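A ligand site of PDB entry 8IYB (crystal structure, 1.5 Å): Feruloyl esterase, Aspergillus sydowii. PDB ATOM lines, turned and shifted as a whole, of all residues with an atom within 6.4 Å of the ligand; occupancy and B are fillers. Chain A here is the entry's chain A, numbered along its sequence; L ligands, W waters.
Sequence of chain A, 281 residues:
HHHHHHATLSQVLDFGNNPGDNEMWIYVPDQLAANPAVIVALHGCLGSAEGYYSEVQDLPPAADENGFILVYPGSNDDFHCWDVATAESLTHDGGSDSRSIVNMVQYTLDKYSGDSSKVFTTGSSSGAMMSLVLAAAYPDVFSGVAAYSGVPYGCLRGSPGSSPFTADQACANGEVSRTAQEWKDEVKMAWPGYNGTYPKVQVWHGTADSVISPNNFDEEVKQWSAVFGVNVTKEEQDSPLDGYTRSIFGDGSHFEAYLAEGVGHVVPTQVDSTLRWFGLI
The side-chain amide oxygen of Gln 169 lies within hydrogen-bond range of an oxygen (O3) of the ligand, 2.7 Å away.
The backbone NH (N) of Cys 45 sits at hydrogen-bond distance from an oxygen (O2) of the ligand.
An oxygen (O2) of the ligand is in hydrogen-bond range of the backbone NH (N) of Ser 126 (2.8 Å).
The side-chain amide nitrogen (NE2) of Gln 169 lies within hydrogen-bond range of the backbone carbonyl oxygen (O) of Pro 164, at 3.4 Å.
NE2 of Gln 169 lies within hydrogen-bond range of O of Ser 163, at 3.4 Å.
O of Ala 167 lies within hydrogen-bond range of NE2 of Gln 169 (2.8 Å).
The backbone carbonyl oxygen (O) of Gln 169 sits close to the side-chain amide nitrogen (ND2) of Asn 173 (3.3 Å).
The side-chain sulfur (SG) of Cys 81 is disulfide-bonded to the side-chain sulfur (SG) of Cys 45, at 2.0 Å.
OG of Ser 125 lies close to ND1 of His 265, at 3.2 Å.
The side-chain hydroxyl of Ser 163 sits at hydrogen-bond distance from the backbone NH of Phe 165 (3.0 Å).
Water W2 lies within hydrogen-bond range of O of Asp 168 (2.8 Å), N of Ala 172 (2.9 Å) and O3 of the ligand (2.9 Å).
Merely in contact with the ligand: Ser 125 (3.0 Å), His 265 (3.0 Å), Ala 172 (3.3 Å), Ser 162 (3.4 Å), Val 211 (3.5 Å), Pro 164 (3.5 Å), Ser 163 (3.6 Å), Gly 44 (3.6 Å), Ile 212 (3.7 Å), Met 129 (3.7 Å) and Ala 167 (3.8 Å).
Hydrophobic or aromatic side chains that line the ligand: Met 129, Pro 164, Ala 167, Ala 172, Val 211, Ile 212 and His 265.
The nearest printed residue that does not touch the ligand is Asp 168 (4.4 Å).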
ATOM      1  N   HIS A  43      -9.212 -22.944   9.046  1.00  0.00           N
ATOM      2  CA  HIS A  43     -10.169 -23.985   9.396  1.00  0.00           C
ATOM      3  C   HIS A  43     -11.302 -23.449  10.265  1.00  0.00           C
ATOM      4  O   HIS A  43     -11.228 -22.371  10.864  1.00  0.00           O
ATOM      5  CB  HIS A  43      -9.462 -25.154  10.101  1.00  0.00           C
ATOM      6  CG  HIS A  43      -8.938 -24.849  11.479  1.00  0.00           C
ATOM      7  ND1 HIS A  43      -9.749 -24.819  12.598  1.00  0.00           N
ATOM      8  CD2 HIS A  43      -7.680 -24.630  11.919  1.00  0.00           C
ATOM      9  CE1 HIS A  43      -9.006 -24.566  13.666  1.00  0.00           C
ATOM     10  NE2 HIS A  43      -7.756 -24.438  13.279  1.00  0.00           N
ATOM     11  N   GLY A  44     -12.367 -24.246  10.337  1.00  0.00           N
ATOM     12  CA  GLY A  44     -13.508 -23.911  11.176  1.00  0.00           C
ATOM     13  C   GLY A  44     -13.395 -24.517  12.560  1.00  0.00           C
ATOM     14  O   GLY A  44     -12.450 -25.223  12.903  1.00  0.00           O
ATOM     15  N   CYS A  45     -14.415 -24.219  13.380  1.00  0.00           N
ATOM     16  CA  CYS A  45     -14.460 -24.744  14.734  1.00  0.00           C
ATOM     17  C   CYS A  45     -14.389 -26.259  14.717  1.00  0.00           C
ATOM     18  O   CYS A  45     -14.894 -26.927  13.795  1.00  0.00           O
ATOM     19  CB  CYS A  45     -15.756 -24.319  15.443  1.00  0.00           C
ATOM     20  SG  CYS A  45     -15.711 -22.646  16.171  1.00  0.00           S
ATOM     21  N   LEU A  46     -13.743 -26.813  15.736  1.00  0.00           N
ATOM     22  CA  LEU A  46     -13.566 -28.248  15.919  1.00  0.00           C
ATOM     23  C   LEU A  46     -12.677 -28.861  14.845  1.00  0.00           C
ATOM     24  O   LEU A  46     -12.574 -30.093  14.762  1.00  0.00           O
ATOM     25  CB  LEU A  46     -14.899 -29.002  16.020  1.00  0.00           C
ATOM     26  CG  LEU A  46     -15.893 -28.503  17.075  1.00  0.00           C
ATOM     27  CD1 LEU A  46     -17.267 -29.134  16.869  1.00  0.00           C
ATOM     28  CD2 LEU A  46     -15.365 -28.807  18.474  1.00  0.00           C
ATOM     29  N   CYS A  81     -11.428 -23.127  17.776  1.00  0.00           N
ATOM     30  CA  CYS A  81     -12.056 -22.010  17.090  1.00  0.00           C
ATOM     31  C   CYS A  81     -11.133 -20.807  17.116  1.00  0.00           C
ATOM     32  O   CYS A  81     -10.269 -20.670  17.984  1.00  0.00           O
ATOM     33  CB  CYS A  81     -13.366 -21.633  17.779  1.00  0.00           C
ATOM     34  SG  CYS A  81     -14.591 -22.964  17.847  1.00  0.00           S
ATOM     35  N   SER A 124     -13.514 -20.912   6.381  1.00  0.00           N
ATOM     36  CA  SER A 124     -14.870 -21.431   6.475  1.00  0.00           C
ATOM     37  C   SER A 124     -15.357 -21.307   7.909  1.00  0.00           C
ATOM     38  O   SER A 124     -14.630 -21.643   8.856  1.00  0.00           O
ATOM     39  CB  SER A 124     -14.921 -22.889   6.028  1.00  0.00           C
ATOM     40  OG  SER A 124     -14.485 -22.997   4.684  1.00  0.00           O
ATOM     41  N   SER A 125     -16.600 -20.835   8.048  1.00  0.00           N
ATOM     42  CA  SER A 125     -17.238 -20.631   9.343  1.00  0.00           C
ATOM     43  C   SER A 125     -16.332 -19.847  10.283  1.00  0.00           C
ATOM     44  O   SER A 125     -16.054 -18.681  10.030  1.00  0.00           O
ATOM     45  CB  SER A 125     -17.659 -21.981   9.923  1.00  0.00           C
ATOM     46  OG  SER A 125     -18.706 -22.520   9.149  1.00  0.00           O
ATOM     47  N   SER A 126     -15.849 -20.473  11.364  1.00  0.00           N
ATOM     48  CA  SER A 126     -14.933 -19.748  12.253  1.00  0.00           C
ATOM     49  C   SER A 126     -13.776 -19.119  11.471  1.00  0.00           C
ATOM     50  O   SER A 126     -13.407 -17.970  11.728  1.00  0.00           O
ATOM     51  CB  SER A 126     -14.387 -20.687  13.331  1.00  0.00           C
ATOM     52  OG  SER A 126     -13.586 -19.950  14.247  1.00  0.00           O
ATOM     53  N   GLY A 127     -13.205 -19.851  10.506  1.00  0.00           N
ATOM     54  CA  GLY A 127     -12.146 -19.294   9.693  1.00  0.00           C
ATOM     55  C   GLY A 127     -12.599 -18.142   8.813  1.00  0.00           C
ATOM     56  O   GLY A 127     -11.807 -17.241   8.507  1.00  0.00           O
ATOM     57  N   MET A 129     -15.016 -16.050   9.817  1.00  0.00           N
ATOM     58  CA  MET A 129     -15.055 -14.960  10.787  1.00  0.00           C
ATOM     59  C   MET A 129     -13.686 -14.325  10.935  1.00  0.00           C
ATOM     60  O   MET A 129     -13.540 -13.100  10.851  1.00  0.00           O
ATOM     61  CB  MET A 129     -15.550 -15.488  12.135  1.00  0.00           C
ATOM     62  CG  MET A 129     -16.917 -16.133  12.050  1.00  0.00           C
ATOM     63  SD  MET A 129     -17.526 -16.649  13.674  1.00  0.00           S
ATOM     64  CE  MET A 129     -18.581 -18.009  13.172  1.00  0.00           C
ATOM     65  N   LEU A 156     -19.073 -10.636  17.569  1.00  0.00           N
ATOM     66  CA  LEU A 156     -18.783 -11.348  18.817  1.00  0.00           C
ATOM     67  C   LEU A 156     -17.897 -10.542  19.769  1.00  0.00           C
ATOM     68  O   LEU A 156     -17.411 -11.097  20.759  1.00  0.00           O
ATOM     69  CB  LEU A 156     -18.192 -12.732  18.527  1.00  0.00           C
ATOM     70  CG  LEU A 156     -19.203 -13.802  18.094  1.00  0.00           C
ATOM     71  CD1 LEU A 156     -18.515 -15.077  17.639  1.00  0.00           C
ATOM     72  CD2 LEU A 156     -20.192 -14.136  19.229  1.00  0.00           C
ATOM     73  N   GLY A 161     -16.560 -16.180  24.476  1.00  0.00           N
ATOM     74  CA  GLY A 161     -15.874 -17.175  23.676  1.00  0.00           C
ATOM     75  C   GLY A 161     -16.270 -17.021  22.230  1.00  0.00           C
ATOM     76  O   GLY A 161     -17.049 -16.129  21.868  1.00  0.00           O
ATOM     77  N   SER A 162     -15.715 -17.899  21.395  1.00  0.00           N
ATOM     78  CA  SER A 162     -15.933 -17.829  19.957  1.00  0.00           C
ATOM     79  C   SER A 162     -16.383 -19.170  19.392  1.00  0.00           C
ATOM     80  O   SER A 162     -16.261 -19.396  18.179  1.00  0.00           O
ATOM     81  CB  SER A 162     -14.664 -17.346  19.230  1.00  0.00           C
ATOM     82  OG  SER A 162     -14.285 -16.037  19.653  1.00  0.00           O
ATOM     83  N   SER A 163     -16.915 -20.055  20.232  1.00  0.00           N
ATOM     84  CA  SER A 163     -17.239 -21.411  19.814  1.00  0.00           C
ATOM     85  C   SER A 163     -18.728 -21.699  20.041  1.00  0.00           C
ATOM     86  O   SER A 163     -19.397 -20.926  20.749  1.00  0.00           O
ATOM     87  CB  SER A 163     -16.398 -22.409  20.619  1.00  0.00           C
ATOM     88  OG  SER A 163     -17.043 -22.774  21.827  1.00  0.00           O
ATOM     89  N   PRO A 164     -19.269 -22.776  19.466  1.00  0.00           N
ATOM     90  CA  PRO A 164     -20.658 -23.161  19.746  1.00  0.00           C
ATOM     91  C   PRO A 164     -20.930 -23.456  21.207  1.00  0.00           C
ATOM     92  O   PRO A 164     -22.104 -23.535  21.596  1.00  0.00           O
ATOM     93  CB  PRO A 164     -20.864 -24.428  18.910  1.00  0.00           C
ATOM     94  CG  PRO A 164     -19.798 -24.356  17.850  1.00  0.00           C
ATOM     95  CD  PRO A 164     -18.634 -23.687  18.488  1.00  0.00           C
ATOM     96  N   PHE A 165     -19.903 -23.608  22.024  1.00  0.00           N
ATOM     97  CA  PHE A 165     -20.057 -24.017  23.417  1.00  0.00           C
ATOM     98  C   PHE A 165     -19.626 -22.948  24.394  1.00  0.00           C
ATOM     99  O   PHE A 165     -19.770 -23.145  25.609  1.00  0.00           O
ATOM    100  CB  PHE A 165     -19.250 -25.308  23.650  1.00  0.00           C
ATOM    101  CG  PHE A 165     -19.365 -26.252  22.514  1.00  0.00           C
ATOM    102  CD1 PHE A 165     -20.504 -27.012  22.343  1.00  0.00           C
ATOM    103  CD2 PHE A 165     -18.373 -26.326  21.552  1.00  0.00           C
ATOM    104  CE1 PHE A 165     -20.640 -27.864  21.273  1.00  0.00           C
ATOM    105  CE2 PHE A 165     -18.493 -27.170  20.470  1.00  0.00           C
ATOM    106  CZ  PHE A 165     -19.637 -27.945  20.333  1.00  0.00           C
ATOM    107  N   ALA A 167     -19.403 -19.148  23.100  1.00  0.00           N
ATOM    108  CA  ALA A 167     -19.793 -17.811  22.693  1.00  0.00           C
ATOM    109  C   ALA A 167     -21.226 -17.491  23.121  1.00  0.00           C
ATOM    110  O   ALA A 167     -22.049 -18.378  23.400  1.00  0.00           O
ATOM    111  CB  ALA A 167     -19.739 -17.686  21.172  1.00  0.00           C
ATOM    112  N   ASP A 168     -21.514 -16.203  23.210  1.00  0.00           N
ATOM    113  CA  ASP A 168     -22.892 -15.746  23.135  1.00  0.00           C
ATOM    114  C   ASP A 168     -23.446 -16.193  21.785  1.00  0.00           C
ATOM    115  O   ASP A 168     -22.851 -15.910  20.743  1.00  0.00           O
ATOM    116  CB  ASP A 168     -22.883 -14.225  23.230  1.00  0.00           C
ATOM    117  CG  ASP A 168     -24.266 -13.612  23.246  1.00  0.00           C
ATOM    118  OD1 ASP A 168     -25.248 -14.258  22.856  1.00  0.00           O
ATOM    119  OD2 ASP A 168     -24.349 -12.430  23.638  1.00  0.00           O
ATOM    120  N   GLN A 169     -24.558 -16.923  21.791  1.00  0.00           N
ATOM    121  CA  GLN A 169     -25.052 -17.530  20.564  1.00  0.00           C
ATOM    122  C   GLN A 169     -25.879 -16.597  19.684  1.00  0.00           C
ATOM    123  O   GLN A 169     -26.320 -17.021  18.615  1.00  0.00           O
ATOM    124  CB  GLN A 169     -25.858 -18.797  20.878  1.00  0.00           C
ATOM    125  CG  GLN A 169     -25.009 -19.874  21.546  1.00  0.00           C
ATOM    126  CD  GLN A 169     -23.790 -20.244  20.731  1.00  0.00           C
ATOM    127  OE1 GLN A 169     -23.907 -20.572  19.547  1.00  0.00           O
ATOM    128  NE2 GLN A 169     -22.614 -20.199  21.356  1.00  0.00           N
ATOM    129  N   ALA A 170     -26.093 -15.346  20.110  1.00  0.00           N
ATOM    130  CA  ALA A 170     -26.932 -14.445  19.310  1.00  0.00           C
ATOM    131  C   ALA A 170     -26.425 -14.313  17.876  1.00  0.00           C
ATOM    132  O   ALA A 170     -27.220 -14.360  16.923  1.00  0.00           O
ATOM    133  CB  ALA A 170     -27.048 -13.088  20.000  1.00  0.00           C
ATOM    134  N   CYS A 171     -25.114 -14.165  17.700  1.00  0.00           N
ATOM    135  CA  CYS A 171     -24.563 -13.993  16.358  1.00  0.00           C
ATOM    136  C   CYS A 171     -24.838 -15.212  15.489  1.00  0.00           C
ATOM    137  O   CYS A 171     -25.430 -15.089  14.413  1.00  0.00           O
ATOM    138  CB  CYS A 171     -23.067 -13.669  16.411  1.00  0.00           C
ATOM    139  SG  CYS A 171     -22.712 -12.029  17.085  1.00  0.00           S
ATOM    140  N   ALA A 172     -24.436 -16.395  15.943  1.00  0.00           N
ATOM    141  CA  ALA A 172     -24.660 -17.613  15.155  1.00  0.00           C
ATOM    142  C   ALA A 172     -26.139 -17.840  14.887  1.00  0.00           C
ATOM    143  O   ALA A 172     -26.501 -18.359  13.819  1.00  0.00           O
ATOM    144  CB  ALA A 172     -24.054 -18.829  15.858  1.00  0.00           C
ATOM    145  N   ASN A 173     -27.001 -17.461  15.822  1.00  0.00           N
ATOM    146  CA  ASN A 173     -28.433 -17.666  15.664  1.00  0.00           C
ATOM    147  C   ASN A 173     -29.062 -16.678  14.712  1.00  0.00           C
ATOM    148  O   ASN A 173     -30.241 -16.832  14.374  1.00  0.00           O
ATOM    149  CB  ASN A 173     -29.124 -17.561  17.026  1.00  0.00           C
ATOM    150  CG  ASN A 173     -28.824 -18.735  17.931  1.00  0.00           C
ATOM    151  OD1 ASN A 173     -28.335 -19.774  17.483  1.00  0.00           O
ATOM    152  ND2 ASN A 173     -29.150 -18.588  19.218  1.00  0.00           N
ATOM    153  N   SER A 210     -27.716 -24.298   9.078  1.00  0.00           N
ATOM    154  CA  SER A 210     -28.281 -24.437  10.413  1.00  0.00           C
ATOM    155  C   SER A 210     -27.283 -24.125  11.522  1.00  0.00           C
ATOM    156  O   SER A 210     -27.657 -24.152  12.703  1.00  0.00           O
ATOM    157  CB  SER A 210     -28.799 -25.869  10.610  1.00  0.00           C
ATOM    158  OG  SER A 210     -27.728 -26.790  10.532  1.00  0.00           O
ATOM    159  N   VAL A 211     -26.037 -23.847  11.179  1.00  0.00           N
ATOM    160  CA  VAL A 211     -24.990 -23.598  12.172  1.00  0.00           C
ATOM    161  C   VAL A 211     -24.797 -22.100  12.343  1.00  0.00           C
ATOM    162  O   VAL A 211     -24.878 -21.572  13.466  1.00  0.00           O
ATOM    163  CB  VAL A 211     -23.674 -24.287  11.769  1.00  0.00           C
ATOM    164  CG1 VAL A 211     -22.571 -23.929  12.748  1.00  0.00           C
ATOM    165  CG2 VAL A 211     -23.875 -25.800  11.704  1.00  0.00           C
ATOM    166  N   ILE A 212     -24.515 -21.406  11.253  1.00  0.00           N
ATOM    167  CA  ILE A 212     -24.414 -19.953  11.226  1.00  0.00           C
ATOM    168  C   ILE A 212     -25.570 -19.437  10.387  1.00  0.00           C
ATOM    169  O   ILE A 212     -25.633 -19.691   9.180  1.00  0.00           O
ATOM    170  CB  ILE A 212     -23.064 -19.496  10.649  1.00  0.00           C
ATOM    171  CG1 ILE A 212     -21.891 -20.081  11.449  1.00  0.00           C
ATOM    172  CG2 ILE A 212     -22.983 -17.972  10.624  1.00  0.00           C
ATOM    173  CD1 ILE A 212     -21.871 -19.685  12.902  1.00  0.00           C
ATOM    174  N   HIS A 265     -24.276 -25.519   6.025  1.00  0.00           N
ATOM    175  CA  HIS A 265     -22.958 -25.316   6.609  1.00  0.00           C
ATOM    176  C   HIS A 265     -22.022 -26.354   5.991  1.00  0.00           C
ATOM    177  O   HIS A 265     -22.247 -27.552   6.173  1.00  0.00           O
ATOM    178  CB  HIS A 265     -23.097 -25.565   8.117  1.00  0.00           C
ATOM    179  CG  HIS A 265     -21.809 -25.773   8.843  1.00  0.00           C
ATOM    180  ND1 HIS A 265     -21.064 -24.734   9.359  1.00  0.00           N
ATOM    181  CD2 HIS A 265     -21.160 -26.916   9.208  1.00  0.00           C
ATOM    182  CE1 HIS A 265     -20.007 -25.219   9.983  1.00  0.00           C
ATOM    183  NE2 HIS A 265     -20.035 -26.538   9.894  1.00  0.00           N
ATOM    184  N   VAL A 266     -21.014 -25.938   5.228  1.00  0.00           N
ATOM    185  CA  VAL A 266     -20.725 -24.572   4.778  1.00  0.00           C
ATOM    186  C   VAL A 266     -20.804 -24.554   3.260  1.00  0.00           C
ATOM    187  O   VAL A 266     -20.924 -25.601   2.623  1.00  0.00           O
ATOM    188  CB  VAL A 266     -19.303 -24.136   5.199  1.00  0.00           C
ATOM    189  CG1 VAL A 266     -19.138 -24.171   6.694  1.00  0.00           C
ATOM    190  CG2 VAL A 266     -18.245 -25.007   4.534  1.00  0.00           C
HETATM  191  C1  LIG L   1     -20.936 -20.040  17.460  1.00  0.00           C
HETATM  192  C2  LIG L   1     -19.666 -19.534  17.199  1.00  0.00           C
HETATM  193  C3  LIG L   1     -18.884 -20.106  16.219  1.00  0.00           C
HETATM  194  C4  LIG L   1     -21.414 -21.118  16.713  1.00  0.00           C
HETATM  195  C5  LIG L   1     -20.627 -21.683  15.727  1.00  0.00           C
HETATM  196  C6  LIG L   1     -19.358 -21.177  15.465  1.00  0.00           C
HETATM  197  C7  LIG L   1     -23.222 -22.633  16.321  1.00  0.00           C
HETATM  198  C8  LIG L   1     -18.507 -21.783  14.443  1.00  0.00           C
HETATM  199  C9  LIG L   1     -18.725 -22.922  13.785  1.00  0.00           C
HETATM  200  C10 LIG L   1     -17.748 -23.443  12.819  1.00  0.00           C
HETATM  201  O1  LIG L   1     -18.060 -24.549  12.217  1.00  0.00           O
HETATM  202  O2  LIG L   1     -16.676 -22.862  12.634  1.00  0.00           O
HETATM  203  O3  LIG L   1     -21.715 -19.495  18.427  1.00  0.00           O
HETATM  204  O4  LIG L   1     -22.673 -21.544  17.053  1.00  0.00           O
HETATM  205  O   HOH W   1     -19.524 -26.515  13.603  1.00  0.00           O
HETATM  206  O   HOH W   2     -22.614 -16.780  18.130  1.00  0.00           O
HETATM  207  O   HOH W   3     -26.498 -22.448  15.473  1.00  0.00           O
HETATM  208  O   HOH W   4     -16.444 -25.804  10.493  1.00  0.00           O
